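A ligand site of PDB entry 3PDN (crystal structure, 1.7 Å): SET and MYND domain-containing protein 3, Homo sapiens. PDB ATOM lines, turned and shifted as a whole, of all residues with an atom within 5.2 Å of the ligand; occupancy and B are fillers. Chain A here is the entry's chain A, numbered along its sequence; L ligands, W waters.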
ATOM      1  N   ASN A  13      -6.134   6.040  25.021  1.00  0.00           N
ATOM      2  CA  ASN A  13      -6.522   5.603  23.663  1.00  0.00           C
ATOM      3  C   ASN A  13      -6.284   6.619  22.550  1.00  0.00           C
ATOM      4  O   ASN A  13      -6.881   6.489  21.474  1.00  0.00           O
ATOM      5  CB  ASN A  13      -8.006   5.186  23.640  1.00  0.00           C
ATOM      6  CG  ASN A  13      -8.992   6.247  24.051  1.00  0.00           C
ATOM      7  OD1 ASN A  13      -8.772   7.454  23.875  1.00  0.00           O
ATOM      8  ND2 ASN A  13     -10.116   5.823  24.611  1.00  0.00           N
ATOM      9  N   ARG A  14      -5.436   7.616  22.783  1.00  0.00           N
ATOM     10  CA  ARG A  14      -5.160   8.565  21.702  1.00  0.00           C
ATOM     11  C   ARG A  14      -3.667   8.895  21.624  1.00  0.00           C
ATOM     12  O   ARG A  14      -3.306  10.006  21.247  1.00  0.00           O
ATOM     13  CB  ARG A  14      -6.031   9.835  21.777  1.00  0.00           C
ATOM     14  CG  ARG A  14      -6.398  10.375  23.138  1.00  0.00           C
ATOM     15  CD  ARG A  14      -7.471  11.417  22.891  1.00  0.00           C
ATOM     16  NE  ARG A  14      -7.829  12.147  24.105  1.00  0.00           N
ATOM     17  CZ  ARG A  14      -8.713  13.149  24.141  1.00  0.00           C
ATOM     18  NH1 ARG A  14      -9.314  13.555  23.021  1.00  0.00           N
ATOM     19  NH2 ARG A  14      -8.971  13.769  25.273  1.00  0.00           N
ATOM     20  N   GLY A  15      -2.835   7.908  21.899  1.00  0.00           N
ATOM     21  CA  GLY A  15      -1.386   8.073  21.807  1.00  0.00           C
ATOM     22  C   GLY A  15      -0.845   8.996  22.870  1.00  0.00           C
ATOM     23  O   GLY A  15      -1.366   9.021  23.982  1.00  0.00           O
ATOM     24  N   ASN A  16       0.205   9.765  22.534  1.00  0.00           N
ATOM     25  CA  ASN A  16       0.720  10.740  23.491  1.00  0.00           C
ATOM     26  C   ASN A  16      -0.177  11.971  23.488  1.00  0.00           C
ATOM     27  O   ASN A  16      -0.891  12.202  22.508  1.00  0.00           O
ATOM     28  CB  ASN A  16       2.172  11.135  23.130  1.00  0.00           C
ATOM     29  CG  ASN A  16       3.097   9.957  23.208  1.00  0.00           C
ATOM     30  OD1 ASN A  16       3.864   9.661  22.260  1.00  0.00           O
ATOM     31  ND2 ASN A  16       2.971   9.195  24.287  1.00  0.00           N
ATOM     32  N   GLY A  17      -0.133  12.721  24.588  1.00  0.00           N
ATOM     33  CA  GLY A  17      -0.884  13.968  24.682  1.00  0.00           C
ATOM     34  C   GLY A  17      -0.192  14.940  25.605  1.00  0.00           C
ATOM     35  O   GLY A  17       0.916  14.682  26.095  1.00  0.00           O
ATOM     36  N   TYR A 124       8.652  17.346  22.326  1.00  0.00           N
ATOM     37  CA  TYR A 124       8.395  16.289  21.343  1.00  0.00           C
ATOM     38  C   TYR A 124       9.113  16.647  20.078  1.00  0.00           C
ATOM     39  O   TYR A 124       9.093  17.809  19.691  1.00  0.00           O
ATOM     40  CB  TYR A 124       6.879  16.256  21.085  1.00  0.00           C
ATOM     41  CG  TYR A 124       6.221  14.938  20.683  1.00  0.00           C
ATOM     42  CD1 TYR A 124       6.423  13.783  21.432  1.00  0.00           C
ATOM     43  CD2 TYR A 124       5.242  14.910  19.685  1.00  0.00           C
ATOM     44  CE1 TYR A 124       5.719  12.608  21.170  1.00  0.00           C
ATOM     45  CE2 TYR A 124       4.558  13.725  19.393  1.00  0.00           C
ATOM     46  CZ  TYR A 124       4.776  12.585  20.151  1.00  0.00           C
ATOM     47  OH  TYR A 124       4.067  11.439  19.901  1.00  0.00           O
ATOM     48  N   ASP A 128       9.662  11.836  16.922  1.00  0.00           N
ATOM     49  CA  ASP A 128       8.625  11.274  17.789  1.00  0.00           C
ATOM     50  C   ASP A 128       7.208  11.343  17.212  1.00  0.00           C
ATOM     51  O   ASP A 128       6.312  10.677  17.733  1.00  0.00           O
ATOM     52  CB  ASP A 128       8.605  12.095  19.094  1.00  0.00           C
ATOM     53  CG  ASP A 128       9.831  12.051  19.983  1.00  0.00           C
ATOM     54  OD1 ASP A 128      10.457  10.960  20.094  1.00  0.00           O
ATOM     55  OD2 ASP A 128      10.082  13.054  20.698  1.00  0.00           O
ATOM     56  N   LEU A 129       6.988  12.191  16.194  1.00  0.00           N
ATOM     57  CA  LEU A 129       5.647  12.452  15.680  1.00  0.00           C
ATOM     58  C   LEU A 129       4.926  11.218  15.214  1.00  0.00           C
ATOM     59  O   LEU A 129       5.528  10.277  14.705  1.00  0.00           O
ATOM     60  CB  LEU A 129       5.653  13.473  14.530  1.00  0.00           C
ATOM     61  CG  LEU A 129       6.150  14.870  14.871  1.00  0.00           C
ATOM     62  CD1 LEU A 129       6.146  15.733  13.607  1.00  0.00           C
ATOM     63  CD2 LEU A 129       5.301  15.521  15.966  1.00  0.00           C
ATOM     64  N   GLU A 130       3.613  11.234  15.440  1.00  0.00           N
ATOM     65  CA  GLU A 130       2.712  10.170  15.037  1.00  0.00           C
ATOM     66  C   GLU A 130       2.670  10.079  13.506  1.00  0.00           C
ATOM     67  O   GLU A 130       2.463  11.088  12.840  1.00  0.00           O
ATOM     68  CB  GLU A 130       1.303  10.441  15.586  1.00  0.00           C
ATOM     69  CG  GLU A 130       0.296   9.393  15.113  1.00  0.00           C
ATOM     70  CD  GLU A 130       0.561   8.004  15.657  1.00  0.00           C
ATOM     71  OE1 GLU A 130       0.341   7.800  16.875  1.00  0.00           O
ATOM     72  OE2 GLU A 130       1.018   7.139  14.887  1.00  0.00           O
ATOM     73  N   ASN A 132       0.738   7.300  11.969  1.00  0.00           N
ATOM     74  CA  ASN A 132      -0.489   6.531  11.657  1.00  0.00           C
ATOM     75  C   ASN A 132      -0.272   5.578  10.482  1.00  0.00           C
ATOM     76  O   ASN A 132      -1.224   5.250   9.776  1.00  0.00           O
ATOM     77  CB  ASN A 132      -1.674   7.452  11.367  1.00  0.00           C
ATOM     78  CG  ASN A 132      -2.194   8.057  12.637  1.00  0.00           C
ATOM     79  OD1 ASN A 132      -2.327   7.390  13.654  1.00  0.00           O
ATOM     80  ND2 ASN A 132      -2.374   9.355  12.624  1.00  0.00           N
ATOM     81  N   CYS A 180      -0.536  14.399   9.221  1.00  0.00           N
ATOM     82  CA  CYS A 180      -1.334  14.540  10.436  1.00  0.00           C
ATOM     83  C   CYS A 180      -0.693  15.456  11.506  1.00  0.00           C
ATOM     84  O   CYS A 180      -1.215  15.525  12.611  1.00  0.00           O
ATOM     85  CB  CYS A 180      -1.670  13.176  11.020  1.00  0.00           C
ATOM     86  SG  CYS A 180      -0.232  12.232  11.561  1.00  0.00           S
ATOM     87  N   ASN A 181       0.373  16.199  11.173  1.00  0.00           N
ATOM     88  CA  ASN A 181       1.010  17.112  12.128  1.00  0.00           C
ATOM     89  C   ASN A 181       1.261  18.517  11.557  1.00  0.00           C
ATOM     90  O   ASN A 181       1.934  19.312  12.204  1.00  0.00           O
ATOM     91  CB  ASN A 181       2.316  16.509  12.661  1.00  0.00           C
ATOM     92  CG  ASN A 181       2.054  15.281  13.507  1.00  0.00           C
ATOM     93  OD1 ASN A 181       1.540  15.379  14.653  1.00  0.00           O
ATOM     94  ND2 ASN A 181       2.324  14.104  12.939  1.00  0.00           N
ATOM     95  N   SER A 202       2.428  19.624  18.544  1.00  0.00           N
ATOM     96  CA  SER A 202       1.761  18.456  17.939  1.00  0.00           C
ATOM     97  C   SER A 202       1.373  17.425  18.998  1.00  0.00           C
ATOM     98  O   SER A 202       0.649  16.505  18.658  1.00  0.00           O
ATOM     99  CB  SER A 202       2.642  17.814  16.868  1.00  0.00           C
ATOM    100  OG  SER A 202       2.610  18.665  15.738  1.00  0.00           O
ATOM    101  N   LEU A 203       1.780  17.601  20.274  1.00  0.00           N
ATOM    102  CA  LEU A 203       1.311  16.674  21.307  1.00  0.00           C
ATOM    103  C   LEU A 203      -0.186  16.866  21.612  1.00  0.00           C
ATOM    104  O   LEU A 203      -0.820  15.969  22.167  1.00  0.00           O
ATOM    105  CB  LEU A 203       2.094  16.868  22.612  1.00  0.00           C
ATOM    106  CG  LEU A 203       3.395  16.120  22.718  1.00  0.00           C
ATOM    107  CD1 LEU A 203       4.221  16.654  23.903  1.00  0.00           C
ATOM    108  CD2 LEU A 203       3.141  14.606  22.840  1.00  0.00           C
ATOM    109  N   LEU A 204      -0.741  18.034  21.278  1.00  0.00           N
ATOM    110  CA  LEU A 204      -2.136  18.297  21.589  1.00  0.00           C
ATOM    111  C   LEU A 204      -3.082  17.462  20.759  1.00  0.00           C
ATOM    112  O   LEU A 204      -3.080  17.564  19.520  1.00  0.00           O
ATOM    113  CB  LEU A 204      -2.477  19.782  21.391  1.00  0.00           C
ATOM    114  CG  LEU A 204      -1.822  20.743  22.362  1.00  0.00           C
ATOM    115  CD1 LEU A 204      -1.614  22.103  21.703  1.00  0.00           C
ATOM    116  CD2 LEU A 204      -2.655  20.927  23.627  1.00  0.00           C
ATOM    117  N   ASN A 205      -3.925  16.658  21.443  1.00  0.00           N
ATOM    118  CA  ASN A 205      -4.967  15.917  20.736  1.00  0.00           C
ATOM    119  C   ASN A 205      -6.148  16.853  20.427  1.00  0.00           C
ATOM    120  O   ASN A 205      -6.243  17.953  20.947  1.00  0.00           O
ATOM    121  CB  ASN A 205      -5.399  14.682  21.557  1.00  0.00           C
ATOM    122  CG  ASN A 205      -4.330  13.618  21.477  1.00  0.00           C
ATOM    123  OD1 ASN A 205      -3.857  13.269  20.380  1.00  0.00           O
ATOM    124  ND2 ASN A 205      -3.914  13.094  22.617  1.00  0.00           N
ATOM    125  N   HIS A 206      -7.023  16.411  19.551  1.00  0.00           N
ATOM    126  CA  HIS A 206      -8.202  17.130  19.061  1.00  0.00           C
ATOM    127  C   HIS A 206      -9.415  17.004  19.959  1.00  0.00           C
ATOM    128  O   HIS A 206      -9.711  15.916  20.477  1.00  0.00           O
ATOM    129  CB  HIS A 206      -8.594  16.523  17.681  1.00  0.00           C
ATOM    130  CG  HIS A 206      -9.935  17.008  17.184  1.00  0.00           C
ATOM    131  ND1 HIS A 206     -10.070  18.240  16.578  1.00  0.00           N
ATOM    132  CD2 HIS A 206     -11.157  16.431  17.279  1.00  0.00           C
ATOM    133  CE1 HIS A 206     -11.369  18.377  16.316  1.00  0.00           C
ATOM    134  NE2 HIS A 206     -12.065  17.324  16.750  1.00  0.00           N
ATOM    135  N   SER A 207     -10.213  18.078  20.016  1.00  0.00           N
ATOM    136  CA  SER A 207     -11.534  18.067  20.574  1.00  0.00           C
ATOM    137  C   SER A 207     -12.427  18.945  19.727  1.00  0.00           C
ATOM    138  O   SER A 207     -11.995  20.016  19.293  1.00  0.00           O
ATOM    139  CB  SER A 207     -11.564  18.535  22.026  1.00  0.00           C
ATOM    140  OG  SER A 207     -12.908  18.610  22.470  1.00  0.00           O
ATOM    141  N   TYR A 239      -8.776  20.761  15.782  1.00  0.00           N
ATOM    142  CA  TYR A 239      -7.987  20.791  14.561  1.00  0.00           C
ATOM    143  C   TYR A 239      -8.708  21.412  13.376  1.00  0.00           C
ATOM    144  O   TYR A 239      -8.062  21.713  12.344  1.00  0.00           O
ATOM    145  CB  TYR A 239      -7.631  19.350  14.149  1.00  0.00           C
ATOM    146  CG  TYR A 239      -6.744  18.536  15.057  1.00  0.00           C
ATOM    147  CD1 TYR A 239      -6.188  19.091  16.222  1.00  0.00           C
ATOM    148  CD2 TYR A 239      -6.395  17.217  14.738  1.00  0.00           C
ATOM    149  CE1 TYR A 239      -5.370  18.338  17.061  1.00  0.00           C
ATOM    150  CE2 TYR A 239      -5.527  16.478  15.545  1.00  0.00           C
ATOM    151  CZ  TYR A 239      -5.022  17.046  16.711  1.00  0.00           C
ATOM    152  OH  TYR A 239      -4.174  16.300  17.509  1.00  0.00           O
ATOM    153  N   GLN A 256      -7.430  12.767   7.135  1.00  0.00           N
ATOM    154  CA  GLN A 256      -6.171  13.424   7.478  1.00  0.00           C
ATOM    155  C   GLN A 256      -5.536  12.875   8.753  1.00  0.00           C
ATOM    156  O   GLN A 256      -4.305  12.754   8.831  1.00  0.00           O
ATOM    157  CB  GLN A 256      -6.397  14.942   7.603  1.00  0.00           C
ATOM    158  CG  GLN A 256      -5.102  15.706   7.843  1.00  0.00           C
ATOM    159  CD  GLN A 256      -5.257  17.204   7.922  1.00  0.00           C
ATOM    160  OE1 GLN A 256      -6.295  17.779   7.573  1.00  0.00           O
ATOM    161  NE2 GLN A 256      -4.197  17.866   8.371  1.00  0.00           N
ATOM    162  N   TYR A 257      -6.351  12.545   9.763  1.00  0.00           N
ATOM    163  CA  TYR A 257      -5.803  12.205  11.081  1.00  0.00           C
ATOM    164  C   TYR A 257      -6.036  10.753  11.522  1.00  0.00           C
ATOM    165  O   TYR A 257      -5.577  10.353  12.606  1.00  0.00           O
ATOM    166  CB  TYR A 257      -6.422  13.148  12.114  1.00  0.00           C
ATOM    167  CG  TYR A 257      -6.082  14.600  11.846  1.00  0.00           C
ATOM    168  CD1 TYR A 257      -4.820  15.110  12.171  1.00  0.00           C
ATOM    169  CD2 TYR A 257      -7.015  15.470  11.277  1.00  0.00           C
ATOM    170  CE1 TYR A 257      -4.509  16.444  11.961  1.00  0.00           C
ATOM    171  CE2 TYR A 257      -6.700  16.817  11.062  1.00  0.00           C
ATOM    172  CZ  TYR A 257      -5.452  17.297  11.403  1.00  0.00           C
ATOM    173  OH  TYR A 257      -5.133  18.613  11.190  1.00  0.00           O
ATOM    174  N   CYS A 258      -6.692   9.955  10.673  1.00  0.00           N
ATOM    175  CA  CYS A 258      -6.930   8.529  10.954  1.00  0.00           C
ATOM    176  C   CYS A 258      -7.541   8.290  12.334  1.00  0.00           C
ATOM    177  O   CYS A 258      -7.076   7.394  13.037  1.00  0.00           O
ATOM    178  CB  CYS A 258      -5.664   7.706  10.781  1.00  0.00           C
ATOM    179  SG  CYS A 258      -5.021   7.695   9.092  1.00  0.00           S
ATOM    180  N   PHE A 259      -8.601   9.027  12.702  1.00  0.00           N
ATOM    181  CA  PHE A 259      -9.319   8.655  13.929  1.00  0.00           C
ATOM    182  C   PHE A 259     -10.799   8.972  13.796  1.00  0.00           C
ATOM    183  O   PHE A 259     -11.201   9.807  12.954  1.00  0.00           O
ATOM    184  CB  PHE A 259      -8.721   9.213  15.231  1.00  0.00           C
ATOM    185  CG  PHE A 259      -8.961  10.684  15.470  1.00  0.00           C
ATOM    186  CD1 PHE A 259     -10.052  11.117  16.223  1.00  0.00           C
ATOM    187  CD2 PHE A 259      -8.096  11.643  14.942  1.00  0.00           C
ATOM    188  CE1 PHE A 259     -10.283  12.488  16.430  1.00  0.00           C
ATOM    189  CE2 PHE A 259      -8.328  13.012  15.164  1.00  0.00           C
ATOM    190  CZ  PHE A 259      -9.408  13.417  15.912  1.00  0.00           C
ATOM    191  N   GLU A 260     -11.596   8.297  14.647  1.00  0.00           N
ATOM    192  CA  GLU A 260     -13.054   8.410  14.809  1.00  0.00           C
ATOM    193  C   GLU A 260     -13.316   9.155  16.084  1.00  0.00           C
ATOM    194  O   GLU A 260     -12.724   8.813  17.122  1.00  0.00           O
ATOM    195  CB  GLU A 260     -13.676   7.002  14.888  1.00  0.00           C
ATOM    196  CG  GLU A 260     -13.090   5.974  13.897  1.00  0.00           C
ATOM    197  CD  GLU A 260     -13.332   6.273  12.425  1.00  0.00           C
ATOM    198  OE1 GLU A 260     -14.172   7.143  12.122  1.00  0.00           O
ATOM    199  OE2 GLU A 260     -12.742   5.557  11.582  1.00  0.00           O
HETATM  200  N1  LIG L   1      -1.633  11.619  19.823  1.00  0.00           N
HETATM  201  C1  LIG L   1      -0.601  12.254  18.961  1.00  0.00           C
HETATM  202  C2  LIG L   1       0.747  11.547  19.247  1.00  0.00           C
HETATM  203  O1  LIG L   1       0.832  10.481  19.909  1.00  0.00           O
HETATM  204  O2  LIG L   1       1.779  12.070  18.724  1.00  0.00           O
HETATM  205  C3  LIG L   1      -0.559  13.769  19.253  1.00  0.00           C
HETATM  206  C4  LIG L   1      -1.584  14.476  18.281  1.00  0.00           C
HETATM  207  C5  LIG L   1      -1.122  14.402  16.694  1.00  0.00           C
HETATM  208  N2  LIG L   1      -0.959  15.809  16.295  1.00  0.00           N
HETATM  209  C6  LIG L   1      -2.434  13.922  15.887  1.00  0.00           C
HETATM  210  C7  LIG L   1      -2.817  12.399  15.962  1.00  0.00           C
HETATM  211  O3  LIG L   1      -3.294  12.155  17.293  1.00  0.00           O
HETATM  212  C8  LIG L   1      -4.043  11.980  15.123  1.00  0.00           C
HETATM  213  O4  LIG L   1      -3.647  11.707  13.787  1.00  0.00           O
HETATM  214  C9  LIG L   1      -4.586  10.700  15.835  1.00  0.00           C
HETATM  215  O5  LIG L   1      -3.634   9.627  15.737  1.00  0.00           O
HETATM  216  C10 LIG L   1      -4.394  11.237  17.308  1.00  0.00           C
HETATM  217  N3  LIG L   1      -5.539  11.967  17.847  1.00  0.00           N
HETATM  218  C11 LIG L   1      -5.617  13.339  18.013  1.00  0.00           C
HETATM  219  N4  LIG L   1      -6.766  13.638  18.598  1.00  0.00           N
HETATM  220  C12 LIG L   1      -7.464  12.446  18.828  1.00  0.00           C
HETATM  221  C13 LIG L   1      -8.730  12.095  19.407  1.00  0.00           C
HETATM  222  N5  LIG L   1      -9.638  13.075  19.898  1.00  0.00           N
HETATM  223  N6  LIG L   1      -9.059  10.784  19.441  1.00  0.00           N
HETATM  224  C14 LIG L   1      -8.251   9.804  18.985  1.00  0.00           C
HETATM  225  N7  LIG L   1      -7.034  10.079  18.421  1.00  0.00           N
HETATM  226  C15 LIG L   1      -6.654  11.385  18.344  1.00  0.00           C
HETATM  227  O   HOH W   1       2.491  13.561  16.514  1.00  0.00           O
HETATM  228  O   HOH W   2       2.204   8.390  18.964  1.00  0.00           O
HETATM  229  O   HOH W   3      -1.822   9.196  18.172  1.00  0.00           O
HETATM  230  O   HOH W   4      -9.632   7.064  20.619  1.00  0.00           O
HETATM  231  O   HOH W   5     -12.490  12.433  20.496  1.00  0.00           O
HETATM  232  O   HOH W   6      -6.123   7.524  17.649  1.00  0.00           O
HETATM  233  O   HOH W   7     -11.787   9.682  20.032  1.00  0.00           O
HETATM  234  O   HOH W   8      -5.136   7.508  14.908  1.00  0.00           O
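N1 of the ligand lies within hydrogen-bond range of O of Asn 16 (2.8 Å). An oxygen (O4) of the ligand sits at hydrogen-bond distance from the side-chain amide nitrogen (ND2) of Asn 132, 2.9 Å away. The side-chain amide oxygen of Asn 181 lies within hydrogen-bond range of a nitrogen (N2) of the ligand (3.0 Å). The backbone carbonyl oxygen (O) of Ser 202 lies within hydrogen-bond range of a nitrogen (N2) of the ligand (2.9 Å). The backbone NH of His 206 sits at hydrogen-bond distance from a nitrogen (N4) of the ligand (2.9 Å). O2 of the ligand sits at hydrogen-bond distance from OH of Tyr 124 (2.6 Å). An oxygen (O1) of the ligand lies within hydrogen-bond range of the backbone NH of Asn 16, 2.8 Å away. O of Arg 14 is in hydrogen-bond range of N1 of the ligand, 2.7 Å away. N1 of the ligand lies within hydrogen-bond range of OD1 of Asn 205 (2.8 Å). The backbone carbonyl oxygen of His 206 is in hydrogen-bond range of a nitrogen (N5) of the ligand, at 2.9 Å. O of Tyr 257 lies within hydrogen-bond range of O4 of the ligand (2.6 Å). OH of Tyr 239 sits close to N2 of the ligand (3.5 Å).
The side-chain amide nitrogen of Asn 132 lies within hydrogen-bond range of the side-chain sulfur of Cys 180, 3.7 Å away. The side-chain amide oxygen (OD1) of Asn 16 is in hydrogen-bond range of the side-chain hydroxyl (OH) of Tyr 124 (3.0 Å). NE2 of Gln 256 lies within hydrogen-bond range of OH of Tyr 257. SG of Cys 180 sits at hydrogen-bond distance from O of Glu 130, at 3.2 Å. The side-chain sulfur of Cys 180 is in hydrogen-bond range of the side-chain amide nitrogen of Asn 181, 3.5 Å away. The backbone carbonyl oxygen of Asp 128 sits at hydrogen-bond distance from the side-chain hydroxyl of Tyr 124, at 3.2 Å. O of Arg 14 lies close to OD1 of Asn 205 (3.4 Å). The backbone carbonyl oxygen (O) of Glu 130 sits at hydrogen-bond distance from the side-chain amide nitrogen (ND2) of Asn 181, 3.0 Å away.
Residues that only touch the ligand: Gly 15 (3.7 Å), Glu 130 (3.6 Å), Cys 180 (3.7 Å), Leu 203 (3.7 Å), Leu 204 (3.6 Å) and Phe 259 (3.4 Å). 16 residues have an atom within 4 Å of the ligand: Arg 14, Gly 15, Asn 16, Tyr 124, Glu 130, Asn 132, Cys 180, Asn 181, Ser 202, Leu 203, Leu 204, Asn 205, His 206, Tyr 239, Tyr 257 and Phe 259. The nearest printed residue that does not touch the ligand is Asn 13 (4.4 Å).
Water W2 lies within hydrogen-bond range of an oxygen (O1) of the ligand (2.7 Å) and the side-chain carboxylate (OE1) of Glu 130 (2.9 Å). Water W8 lies within hydrogen-bond range of O of Cys 258, O5 of the ligand and OD1 of Asn 132. Water W1 lies within hydrogen-bond range of an oxygen (O2) of the ligand (2.8 Å), the side-chain amide oxygen of Asn 181 (2.8 Å) and the backbone NH of Glu 130 (2.8 Å). Water W3 bridges the side-chain carboxylate of Glu 130 and a nitrogen (N1) of the ligand. Water W7 lies within hydrogen-bond range of N6 of the ligand (3.0 Å) and O of Glu 260 (3.2 Å).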
